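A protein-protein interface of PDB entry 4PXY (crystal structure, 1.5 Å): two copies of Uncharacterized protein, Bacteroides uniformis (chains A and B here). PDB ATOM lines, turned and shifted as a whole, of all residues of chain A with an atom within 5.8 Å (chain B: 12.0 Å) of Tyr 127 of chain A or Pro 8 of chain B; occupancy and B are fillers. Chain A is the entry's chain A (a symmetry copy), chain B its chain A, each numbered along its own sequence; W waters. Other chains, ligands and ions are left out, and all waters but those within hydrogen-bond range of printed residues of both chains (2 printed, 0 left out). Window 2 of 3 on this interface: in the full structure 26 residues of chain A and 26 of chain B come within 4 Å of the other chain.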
ATOM      1  N   VAL A 125     -17.281  20.213   9.453  1.00  0.00           N
ATOM      2  CA  VAL A 125     -16.162  19.996   8.538  1.00  0.00           C
ATOM      3  C   VAL A 125     -14.884  20.038   9.398  1.00  0.00           C
ATOM      4  O   VAL A 125     -14.831  20.763  10.404  1.00  0.00           O
ATOM      5  CB  VAL A 125     -16.111  21.118   7.472  1.00  0.00           C
ATOM      6  CG1 VAL A 125     -14.954  20.929   6.508  1.00  0.00           C
ATOM      7  CG2 VAL A 125     -17.436  21.094   6.705  1.00  0.00           C
ATOM      8  N   PHE A 126     -13.886  19.246   9.023  1.00  0.00           N
ATOM      9  CA  PHE A 126     -12.647  19.224   9.846  1.00  0.00           C
ATOM     10  C   PHE A 126     -12.066  20.640  10.009  1.00  0.00           C
ATOM     11  O   PHE A 126     -11.988  21.402   9.040  1.00  0.00           O
ATOM     12  CB  PHE A 126     -11.599  18.299   9.224  1.00  0.00           C
ATOM     13  CG  PHE A 126     -10.283  18.328   9.972  1.00  0.00           C
ATOM     14  CD1 PHE A 126     -10.133  17.572  11.115  1.00  0.00           C
ATOM     15  CD2 PHE A 126      -9.274  19.138   9.576  1.00  0.00           C
ATOM     16  CE1 PHE A 126      -8.975  17.664  11.858  1.00  0.00           C
ATOM     17  CE2 PHE A 126      -8.087  19.204  10.304  1.00  0.00           C
ATOM     18  CZ  PHE A 126      -7.950  18.449  11.450  1.00  0.00           C
ATOM     19  N   TYR A 127     -11.645  20.973  11.227  1.00  0.00           N
ATOM     20  CA  TYR A 127     -11.155  22.288  11.563  1.00  0.00           C
ATOM     21  C   TYR A 127      -9.726  22.270  12.068  1.00  0.00           C
ATOM     22  O   TYR A 127      -8.876  22.993  11.555  1.00  0.00           O
ATOM     23  CB  TYR A 127     -12.083  22.961  12.585  1.00  0.00           C
ATOM     24  CG  TYR A 127     -11.896  24.421  12.882  1.00  0.00           C
ATOM     25  CD1 TYR A 127     -11.695  25.329  11.881  1.00  0.00           C
ATOM     26  CD2 TYR A 127     -12.007  24.885  14.194  1.00  0.00           C
ATOM     27  CE1 TYR A 127     -11.587  26.687  12.149  1.00  0.00           C
ATOM     28  CE2 TYR A 127     -11.904  26.235  14.485  1.00  0.00           C
ATOM     29  CZ  TYR A 127     -11.687  27.124  13.449  1.00  0.00           C
ATOM     30  OH  TYR A 127     -11.558  28.472  13.743  1.00  0.00           O
ATOM     31  N   CYS A 128      -9.456  21.496  13.102  1.00  0.00           N
ATOM     32  CA  CYS A 128      -8.084  21.442  13.637  1.00  0.00           C
ATOM     33  C   CYS A 128      -7.940  20.218  14.521  1.00  0.00           C
ATOM     34  O   CYS A 128      -8.891  19.506  14.784  1.00  0.00           O
ATOM     35  CB  CYS A 128      -7.706  22.682  14.430  1.00  0.00           C
ATOM     36  SG  CYS A 128      -8.463  22.952  16.026  1.00  0.00           S
ATOM     37  N   ASN A 129      -6.693  19.967  14.908  1.00  0.00           N
ATOM     38  CA  ASN A 129      -6.388  18.816  15.787  1.00  0.00           C
ATOM     39  C   ASN A 129      -5.152  19.125  16.615  1.00  0.00           C
ATOM     40  O   ASN A 129      -4.332  19.954  16.218  1.00  0.00           O
ATOM     41  CB  ASN A 129      -6.175  17.555  14.977  1.00  0.00           C
ATOM     42  CG  ASN A 129      -4.954  17.637  14.104  1.00  0.00           C
ATOM     43  OD1 ASN A 129      -4.942  18.359  13.074  1.00  0.00           O
ATOM     44  ND2 ASN A 129      -3.872  16.982  14.523  1.00  0.00           N
ATOM     45  N   GLN A 164     -11.259  18.975  16.235  1.00  0.00           N
ATOM     46  CA  GLN A 164     -12.334  19.962  16.246  1.00  0.00           C
ATOM     47  C   GLN A 164     -12.884  20.120  14.830  1.00  0.00           C
ATOM     48  O   GLN A 164     -12.207  19.843  13.854  1.00  0.00           O
ATOM     49  CB  GLN A 164     -11.856  21.349  16.739  1.00  0.00           C
ATOM     50  CG  GLN A 164     -11.546  21.410  18.207  1.00  0.00           C
ATOM     51  CD  GLN A 164     -11.222  22.836  18.652  1.00  0.00           C
ATOM     52  OE1 GLN A 164     -11.219  23.738  17.816  1.00  0.00           O
ATOM     53  NE2 GLN A 164     -11.081  23.090  19.937  1.00  0.00           N
ATOM     54  N   TRP A 165     -14.136  20.569  14.788  1.00  0.00           N
ATOM     55  CA  TRP A 165     -14.910  20.698  13.584  1.00  0.00           C
ATOM     56  C   TRP A 165     -15.513  22.088  13.508  1.00  0.00           C
ATOM     57  O   TRP A 165     -15.658  22.760  14.526  1.00  0.00           O
ATOM     58  CB  TRP A 165     -16.064  19.678  13.587  1.00  0.00           C
ATOM     59  CG  TRP A 165     -15.624  18.281  13.914  1.00  0.00           C
ATOM     60  CD1 TRP A 165     -15.490  17.733  15.156  1.00  0.00           C
ATOM     61  CD2 TRP A 165     -15.214  17.253  12.993  1.00  0.00           C
ATOM     62  NE1 TRP A 165     -15.025  16.470  15.066  1.00  0.00           N
ATOM     63  CE2 TRP A 165     -14.868  16.118  13.760  1.00  0.00           C
ATOM     64  CE3 TRP A 165     -15.120  17.183  11.611  1.00  0.00           C
ATOM     65  CZ2 TRP A 165     -14.477  14.930  13.184  1.00  0.00           C
ATOM     66  CZ3 TRP A 165     -14.736  16.019  11.029  1.00  0.00           C
ATOM     67  CH2 TRP A 165     -14.410  14.880  11.810  1.00  0.00           C
ATOM     68  N   THR A 166     -15.823  22.543  12.309  1.00  0.00           N
ATOM     69  CA  THR A 166     -16.528  23.820  12.171  1.00  0.00           C
ATOM     70  C   THR A 166     -17.676  23.656  11.187  1.00  0.00           C
ATOM     71  O   THR A 166     -17.478  23.114  10.111  1.00  0.00           O
ATOM     72  CB  THR A 166     -15.580  24.934  11.751  1.00  0.00           C
ATOM     73  OG1 THR A 166     -16.287  26.193  11.734  1.00  0.00           O
ATOM     74  CG2 THR A 166     -14.925  24.656  10.400  1.00  0.00           C
ATOM     75  N   VAL A 193      -0.788  22.733  18.760  1.00  0.00           N
ATOM     76  CA  VAL A 193      -1.405  23.107  20.032  1.00  0.00           C
ATOM     77  C   VAL A 193      -2.772  23.741  19.844  1.00  0.00           C
ATOM     78  O   VAL A 193      -2.897  24.693  19.101  1.00  0.00           O
ATOM     79  CB  VAL A 193      -0.520  24.108  20.792  1.00  0.00           C
ATOM     80  CG1 VAL A 193      -1.092  24.373  22.178  1.00  0.00           C
ATOM     81  CG2 VAL A 193       0.913  23.569  20.871  1.00  0.00           C
ATOM     82  N   VAL A 194      -3.796  23.185  20.478  1.00  0.00           N
ATOM     83  CA  VAL A 194      -5.143  23.690  20.482  1.00  0.00           C
ATOM     84  C   VAL A 194      -5.373  24.432  21.794  1.00  0.00           C
ATOM     85  O   VAL A 194      -5.181  23.887  22.858  1.00  0.00           O
ATOM     86  CB  VAL A 194      -6.178  22.567  20.314  1.00  0.00           C
ATOM     87  CG1 VAL A 194      -7.598  23.139  20.189  1.00  0.00           C
ATOM     88  CG2 VAL A 194      -5.868  21.745  19.062  1.00  0.00           C
ATOM     89  N   ASN A 195      -5.834  25.672  21.678  1.00  0.00           N
ATOM     90  CA  ASN A 195      -5.913  26.580  22.821  1.00  0.00           C
ATOM     91  C   ASN A 195      -7.287  26.881  23.393  1.00  0.00           C
ATOM     92  O   ASN A 195      -7.369  27.305  24.527  1.00  0.00           O
ATOM     93  CB  ASN A 195      -5.239  27.881  22.410  1.00  0.00           C
ATOM     94  CG  ASN A 195      -3.730  27.699  22.241  1.00  0.00           C
ATOM     95  OD1 ASN A 195      -3.072  27.146  23.122  1.00  0.00           O
ATOM     96  ND2 ASN A 195      -3.223  28.079  21.114  1.00  0.00           N
ATOM     97  N   PHE A 196      -8.327  26.656  22.603  1.00  0.00           N
ATOM     98  CA  PHE A 196      -9.686  26.968  23.021  1.00  0.00           C
ATOM     99  C   PHE A 196     -10.655  26.326  22.054  1.00  0.00           C
ATOM    100  O   PHE A 196     -10.268  25.758  21.002  1.00  0.00           O
ATOM    101  CB  PHE A 196      -9.916  28.460  23.154  1.00  0.00           C
ATOM    102  CG  PHE A 196      -9.740  29.214  21.885  1.00  0.00           C
ATOM    103  CD1 PHE A 196     -10.785  29.330  20.983  1.00  0.00           C
ATOM    104  CD2 PHE A 196      -8.529  29.866  21.614  1.00  0.00           C
ATOM    105  CE1 PHE A 196     -10.623  30.030  19.799  1.00  0.00           C
ATOM    106  CE2 PHE A 196      -8.367  30.588  20.458  1.00  0.00           C
ATOM    107  CZ  PHE A 196      -9.411  30.659  19.537  1.00  0.00           C
ATOM    108  N   GLY A 197     -11.918  26.354  22.451  1.00  0.00           N
ATOM    109  CA  GLY A 197     -13.020  25.966  21.570  1.00  0.00           C
ATOM    110  C   GLY A 197     -13.807  24.815  22.125  1.00  0.00           C
ATOM    111  O   GLY A 197     -13.322  24.058  22.951  1.00  0.00           O
ATOM    112  N   TYR B   7      -8.490  31.574  15.180  1.00  0.00           N
ATOM    113  CA  TYR B   7      -8.182  30.122  14.939  1.00  0.00           C
ATOM    114  C   TYR B   7      -7.602  29.539  16.198  1.00  0.00           C
ATOM    115  O   TYR B   7      -6.669  30.103  16.770  1.00  0.00           O
ATOM    116  CB  TYR B   7      -7.213  29.949  13.758  1.00  0.00           C
ATOM    117  CG  TYR B   7      -7.045  28.509  13.280  1.00  0.00           C
ATOM    118  CD1 TYR B   7      -8.142  27.779  12.792  1.00  0.00           C
ATOM    119  CD2 TYR B   7      -5.796  27.880  13.300  1.00  0.00           C
ATOM    120  CE1 TYR B   7      -7.997  26.474  12.339  1.00  0.00           C
ATOM    121  CE2 TYR B   7      -5.641  26.569  12.843  1.00  0.00           C
ATOM    122  CZ  TYR B   7      -6.750  25.877  12.366  1.00  0.00           C
ATOM    123  OH  TYR B   7      -6.621  24.585  11.912  1.00  0.00           O
ATOM    124  N   PRO B   8      -8.133  28.386  16.661  1.00  0.00           N
ATOM    125  CA  PRO B   8      -7.683  28.027  17.994  1.00  0.00           C
ATOM    126  C   PRO B   8      -6.410  27.223  18.057  1.00  0.00           C
ATOM    127  O   PRO B   8      -6.041  26.839  19.169  1.00  0.00           O
ATOM    128  CB  PRO B   8      -8.838  27.149  18.532  1.00  0.00           C
ATOM    129  CG  PRO B   8      -9.439  26.538  17.318  1.00  0.00           C
ATOM    130  CD  PRO B   8      -9.261  27.548  16.209  1.00  0.00           C
ATOM    131  N   ALA B   9      -5.757  26.942  16.910  1.00  0.00           N
ATOM    132  CA  ALA B   9      -4.590  26.041  16.908  1.00  0.00           C
ATOM    133  C   ALA B   9      -3.320  26.688  16.353  1.00  0.00           C
ATOM    134  O   ALA B   9      -3.352  27.431  15.381  1.00  0.00           O
ATOM    135  CB  ALA B   9      -4.897  24.767  16.138  1.00  0.00           C
ATOM    136  N   ASN B  10      -2.204  26.353  16.986  1.00  0.00           N
ATOM    137  CA  ASN B  10      -0.856  26.783  16.586  1.00  0.00           C
ATOM    138  C   ASN B  10      -0.094  25.507  16.152  1.00  0.00           C
ATOM    139  O   ASN B  10       0.314  24.678  16.968  1.00  0.00           O
ATOM    140  CB  ASN B  10      -0.176  27.432  17.773  1.00  0.00           C
ATOM    141  CG  ASN B  10       1.295  27.807  17.523  1.00  0.00           C
ATOM    142  OD1 ASN B  10       1.995  27.197  16.735  1.00  0.00           O
ATOM    143  ND2 ASN B  10       1.765  28.805  18.239  1.00  0.00           N
ATOM    144  N   TYR B  11      -0.001  25.373  14.833  1.00  0.00           N
ATOM    145  CA  TYR B  11       0.695  24.259  14.184  1.00  0.00           C
ATOM    146  C   TYR B  11       2.166  24.593  14.069  1.00  0.00           C
ATOM    147  O   TYR B  11       2.539  25.645  13.508  1.00  0.00           O
ATOM    148  CB  TYR B  11       0.097  23.998  12.816  1.00  0.00           C
ATOM    149  CG  TYR B  11      -1.238  23.221  12.873  1.00  0.00           C
ATOM    150  CD1 TYR B  11      -2.432  23.873  13.038  1.00  0.00           C
ATOM    151  CD2 TYR B  11      -1.263  21.840  12.725  1.00  0.00           C
ATOM    152  CE1 TYR B  11      -3.656  23.162  13.045  1.00  0.00           C
ATOM    153  CE2 TYR B  11      -2.476  21.133  12.764  1.00  0.00           C
ATOM    154  CZ  TYR B  11      -3.647  21.815  12.951  1.00  0.00           C
ATOM    155  OH  TYR B  11      -4.840  21.114  12.982  1.00  0.00           O
ATOM    156  N   ALA B  12       3.017  23.696  14.541  1.00  0.00           N
ATOM    157  CA  ALA B  12       4.472  23.930  14.461  1.00  0.00           C
ATOM    158  C   ALA B  12       4.921  24.009  13.025  1.00  0.00           C
ATOM    159  O   ALA B  12       4.477  23.268  12.173  1.00  0.00           O
ATOM    160  CB  ALA B  12       5.227  22.826  15.168  1.00  0.00           C
ATOM    161  N   ARG B  16      10.171  22.512  17.966  1.00  0.00           N
ATOM    162  CA  ARG B  16       9.991  23.625  18.891  1.00  0.00           C
ATOM    163  C   ARG B  16      11.114  23.801  19.916  1.00  0.00           C
ATOM    164  O   ARG B  16      11.327  24.899  20.443  1.00  0.00           O
ATOM    165  CB  ARG B  16       8.666  23.441  19.638  1.00  0.00           C
ATOM    166  CG  ARG B  16       7.397  23.624  18.787  1.00  0.00           C
ATOM    167  CD  ARG B  16       6.194  23.604  19.686  1.00  0.00           C
ATOM    168  NE  ARG B  16       4.960  23.750  18.954  1.00  0.00           N
ATOM    169  CZ  ARG B  16       4.479  24.914  18.532  1.00  0.00           C
ATOM    170  NH1 ARG B  16       5.105  26.052  18.848  1.00  0.00           N
ATOM    171  NH2 ARG B  16       3.362  24.974  17.792  1.00  0.00           N
ATOM    172  N   ARG B 236       5.542  18.480  29.513  1.00  0.00           N
ATOM    173  CA  ARG B 236       5.092  19.715  28.866  1.00  0.00           C
ATOM    174  C   ARG B 236       5.328  20.928  29.774  1.00  0.00           C
ATOM    175  O   ARG B 236       5.772  22.001  29.322  1.00  0.00           O
ATOM    176  CB  ARG B 236       3.631  19.595  28.508  1.00  0.00           C
ATOM    177  CG  ARG B 236       3.190  20.690  27.565  1.00  0.00           C
ATOM    178  CD  ARG B 236       1.673  20.686  27.325  1.00  0.00           C
ATOM    179  NE  ARG B 236       1.304  21.522  26.201  1.00  0.00           N
ATOM    180  CZ  ARG B 236       1.328  22.867  26.163  1.00  0.00           C
ATOM    181  NH1 ARG B 236       1.577  23.540  27.280  1.00  0.00           N
ATOM    182  NH2 ARG B 236       1.054  23.506  25.040  1.00  0.00           N
ATOM    183  N   PHE B 248       5.956  26.516  23.136  1.00  0.00           N
ATOM    184  CA  PHE B 248       4.640  26.223  22.615  1.00  0.00           C
ATOM    185  C   PHE B 248       3.938  27.442  22.031  1.00  0.00           C
ATOM    186  O   PHE B 248       2.900  27.298  21.378  1.00  0.00           O
ATOM    187  CB  PHE B 248       3.780  25.529  23.679  1.00  0.00           C
ATOM    188  CG  PHE B 248       4.397  24.282  24.160  1.00  0.00           C
ATOM    189  CD1 PHE B 248       4.662  23.273  23.233  1.00  0.00           C
ATOM    190  CD2 PHE B 248       4.873  24.113  25.439  1.00  0.00           C
ATOM    191  CE1 PHE B 248       5.306  22.138  23.596  1.00  0.00           C
ATOM    192  CE2 PHE B 248       5.506  22.931  25.814  1.00  0.00           C
ATOM    193  CZ  PHE B 248       5.739  21.937  24.886  1.00  0.00           C
ATOM    194  N   LEU B 249       4.513  28.627  22.270  1.00  0.00           N
ATOM    195  CA  LEU B 249       4.001  29.867  21.688  1.00  0.00           C
ATOM    196  C   LEU B 249       4.622  30.183  20.326  1.00  0.00           C
ATOM    197  O   LEU B 249       4.142  31.091  19.627  1.00  0.00           O
ATOM    198  CB  LEU B 249       4.242  31.012  22.666  1.00  0.00           C
ATOM    199  CG  LEU B 249       3.501  30.860  24.002  1.00  0.00           C
ATOM    200  CD1 LEU B 249       3.813  32.036  24.930  1.00  0.00           C
ATOM    201  CD2 LEU B 249       1.995  30.760  23.787  1.00  0.00           C
ATOM    202  N   LYS B 250       5.683  29.472  19.930  1.00  0.00           N
ATOM    203  CA  LYS B 250       6.421  29.804  18.680  1.00  0.00           C
ATOM    204  C   LYS B 250       5.552  29.565  17.490  1.00  0.00           C
ATOM    205  O   LYS B 250       4.701  28.650  17.505  1.00  0.00           O
ATOM    206  CB  LYS B 250       7.668  28.930  18.510  1.00  0.00           C
ATOM    207  CG  LYS B 250       8.817  29.222  19.420  1.00  0.00           C
ATOM    208  CD  LYS B 250       9.841  28.062  19.327  1.00  0.00           C
ATOM    209  CE  LYS B 250      11.041  28.381  20.177  1.00  0.00           C
ATOM    210  NZ  LYS B 250      12.138  27.420  19.894  1.00  0.00           N
ATOM    211  OXT LYS B 250       5.689  30.289  16.488  1.00  0.00           O
HETATM  212  O   HOH W   1      -4.562  29.730  19.040  1.00  0.00           O
HETATM  213  O   HOH W   2       0.152  28.094  21.165  1.00  0.00           O
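The backbone carbonyl oxygen (O) of Tyr 127 of chain A lies within hydrogen-bond range of the side-chain hydroxyl (OH) of Tyr 7 of chain B (2.8 Å).
The backbone NH of Asn 195 of chain A lies within hydrogen-bond range of the backbone carbonyl oxygen of Pro 8 of chain B (2.8 Å).
The backbone NH (N) of Asn 10 of chain B sits at hydrogen-bond distance from the backbone carbonyl oxygen (O) of Val 193 of chain A (2.8 Å).
The side-chain amide oxygen of Asn 129 of chain A lies within hydrogen-bond range of the side-chain hydroxyl of Tyr 11 of chain B (2.8 Å).
The guanidinium group (NH2) of Arg 16 of chain B is in hydrogen-bond range of the side-chain amide oxygen (OD1) of Asn 10 of chain B.
The side-chain amide nitrogen of Asn 10 of chain B lies within hydrogen-bond range of the chain-end carboxylate of Lys 250 of chain B, at 3.0 Å.
The backbone NH of Tyr 127 of chain A sits at hydrogen-bond distance from the backbone carbonyl oxygen of Gln 164 of chain A (2.9 Å).
The backbone carbonyl oxygen (O) of Cys 128 of chain A is in hydrogen-bond range of the backbone NH (N) of Gln 164 of chain A, at 2.8 Å.
O of Phe 196 of chain A lies within hydrogen-bond range of NE2 of Gln 164 of chain A, 3.0 Å away.
Tyr 127 of chain A touches Pro 8 of chain B.
Cys 128 of chain A touches Pro 8 of chain B.
CB of Cys 128 of chain A touches CB of Ala 9 of chain B, 3.9 Å away.
OE1 of Gln 164 of chain A touches CG of Pro 8 of chain B, at 3.4 Å.
Val 193 of chain A touches Pro 8 of chain B (O to O, 3.8 Å).
CA of Ala 9 of chain B touches O of Val 193 of chain A, 3.1 Å away.
CG1 of Val 193 of chain A touches NH2 of Arg 236 of chain B, at 3.7 Å.
Val 194 of chain A touches Pro 8 of chain B (CA to O, 3.5 Å).
CZ of Phe 196 of chain A touches O of Tyr 7 of chain B, 3.9 Å away.
Phe 196 of chain A touches Pro 8 of chain B (O to CB, 3.2 Å).
No residue of chain B comes within 4 Å of Phe 126 of chain A.
Of chain B, only Tyr 7 and Pro 8 come within 4 Å of Tyr 127 of chain A.
Of the printed residues of chain B, Cys 128 of chain A touches Tyr 7 (3.3 Å), Pro 8 (3.9 Å), Ala 9 (3.9 Å) and Tyr 11 (3.3 Å).
Printed residues of chain B within 4 Å of Asn 129 of chain A: Tyr 11 (2.8 Å).
Gln 164 of chain A touches just one residue of chain B: Pro 8.
Trp 165 of chain A touches none of the printed residues of chain B.
No residue of chain B comes within 4 Å of Thr 166 of chain A.
Of chain B, only Pro 8 (3.8 Å), Ala 9 (3.1 Å), Asn 10 (2.8 Å) and Arg 236 (3.7 Å) come within 4 Å of Val 193 of chain A.
Of chain B, only Pro 8 (3.5 Å) comes within 4 Å of Val 194 of chain A.
Of the printed residues of chain A, Tyr 7 of chain B touches Tyr 127, Cys 128 and Phe 196.
Pro 8 of chain B touches just these residues of chain A: Tyr 127, Cys 128, Gln 164, Val 193, Val 194, Asn 195 and Phe 196.
Of the printed residues of chain A, Ala 9 of chain B touches Cys 128 and Val 193.
The nearest residue of chain B that does not touch Tyr 127 of chain A is Tyr 11 of chain B (4.7 Å).
The nearest residue of chain A that does not touch Pro 8 of chain B is Gly 197 of chain A (5.0 Å).
The nearest printed residue of chain A that does not touch Arg 236 of chain B is Asn 195 of chain A (5.8 Å).
Printed residues of chain B that touch a printed residue of chain A: Tyr 7, Pro 8, Ala 9, Asn 10, Tyr 11 and Arg 236.
Hydrophobic or aromatic side chains of chain B that line the printed part of chain A: Tyr 7, Pro 8, Ala 9 and Tyr 11.
Hydrophobic or aromatic side chains of chain A within 4 Å of the printed part of chain B: Tyr 127, Val 193 and Phe 196.
Among the printed residues, no Asp or Glu carboxylate lies within 4 Å of a Lys or Arg side-chain nitrogen of the other chain.
No position is printed for both chains.
Of the 16 pairs that touch across the chains among the printed residues, none has its exchanged pair printed and touching as well.
Water W2 lies within hydrogen-bond range of the backbone carbonyl oxygen (O) of Phe 248 of chain B (2.9 Å), the side-chain amide nitrogen (ND2) of Asn 195 of chain A (3.4 Å) and the side-chain amide nitrogen (ND2) of Asn 10 of chain B (3.4 Å).
Water W1 lies within hydrogen-bond range of ND2 of Asn 195 of chain A (3.0 Å), O of Tyr 7 of chain B (3.1 Å) and O of Pro 8 of chain B (3.2 Å).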
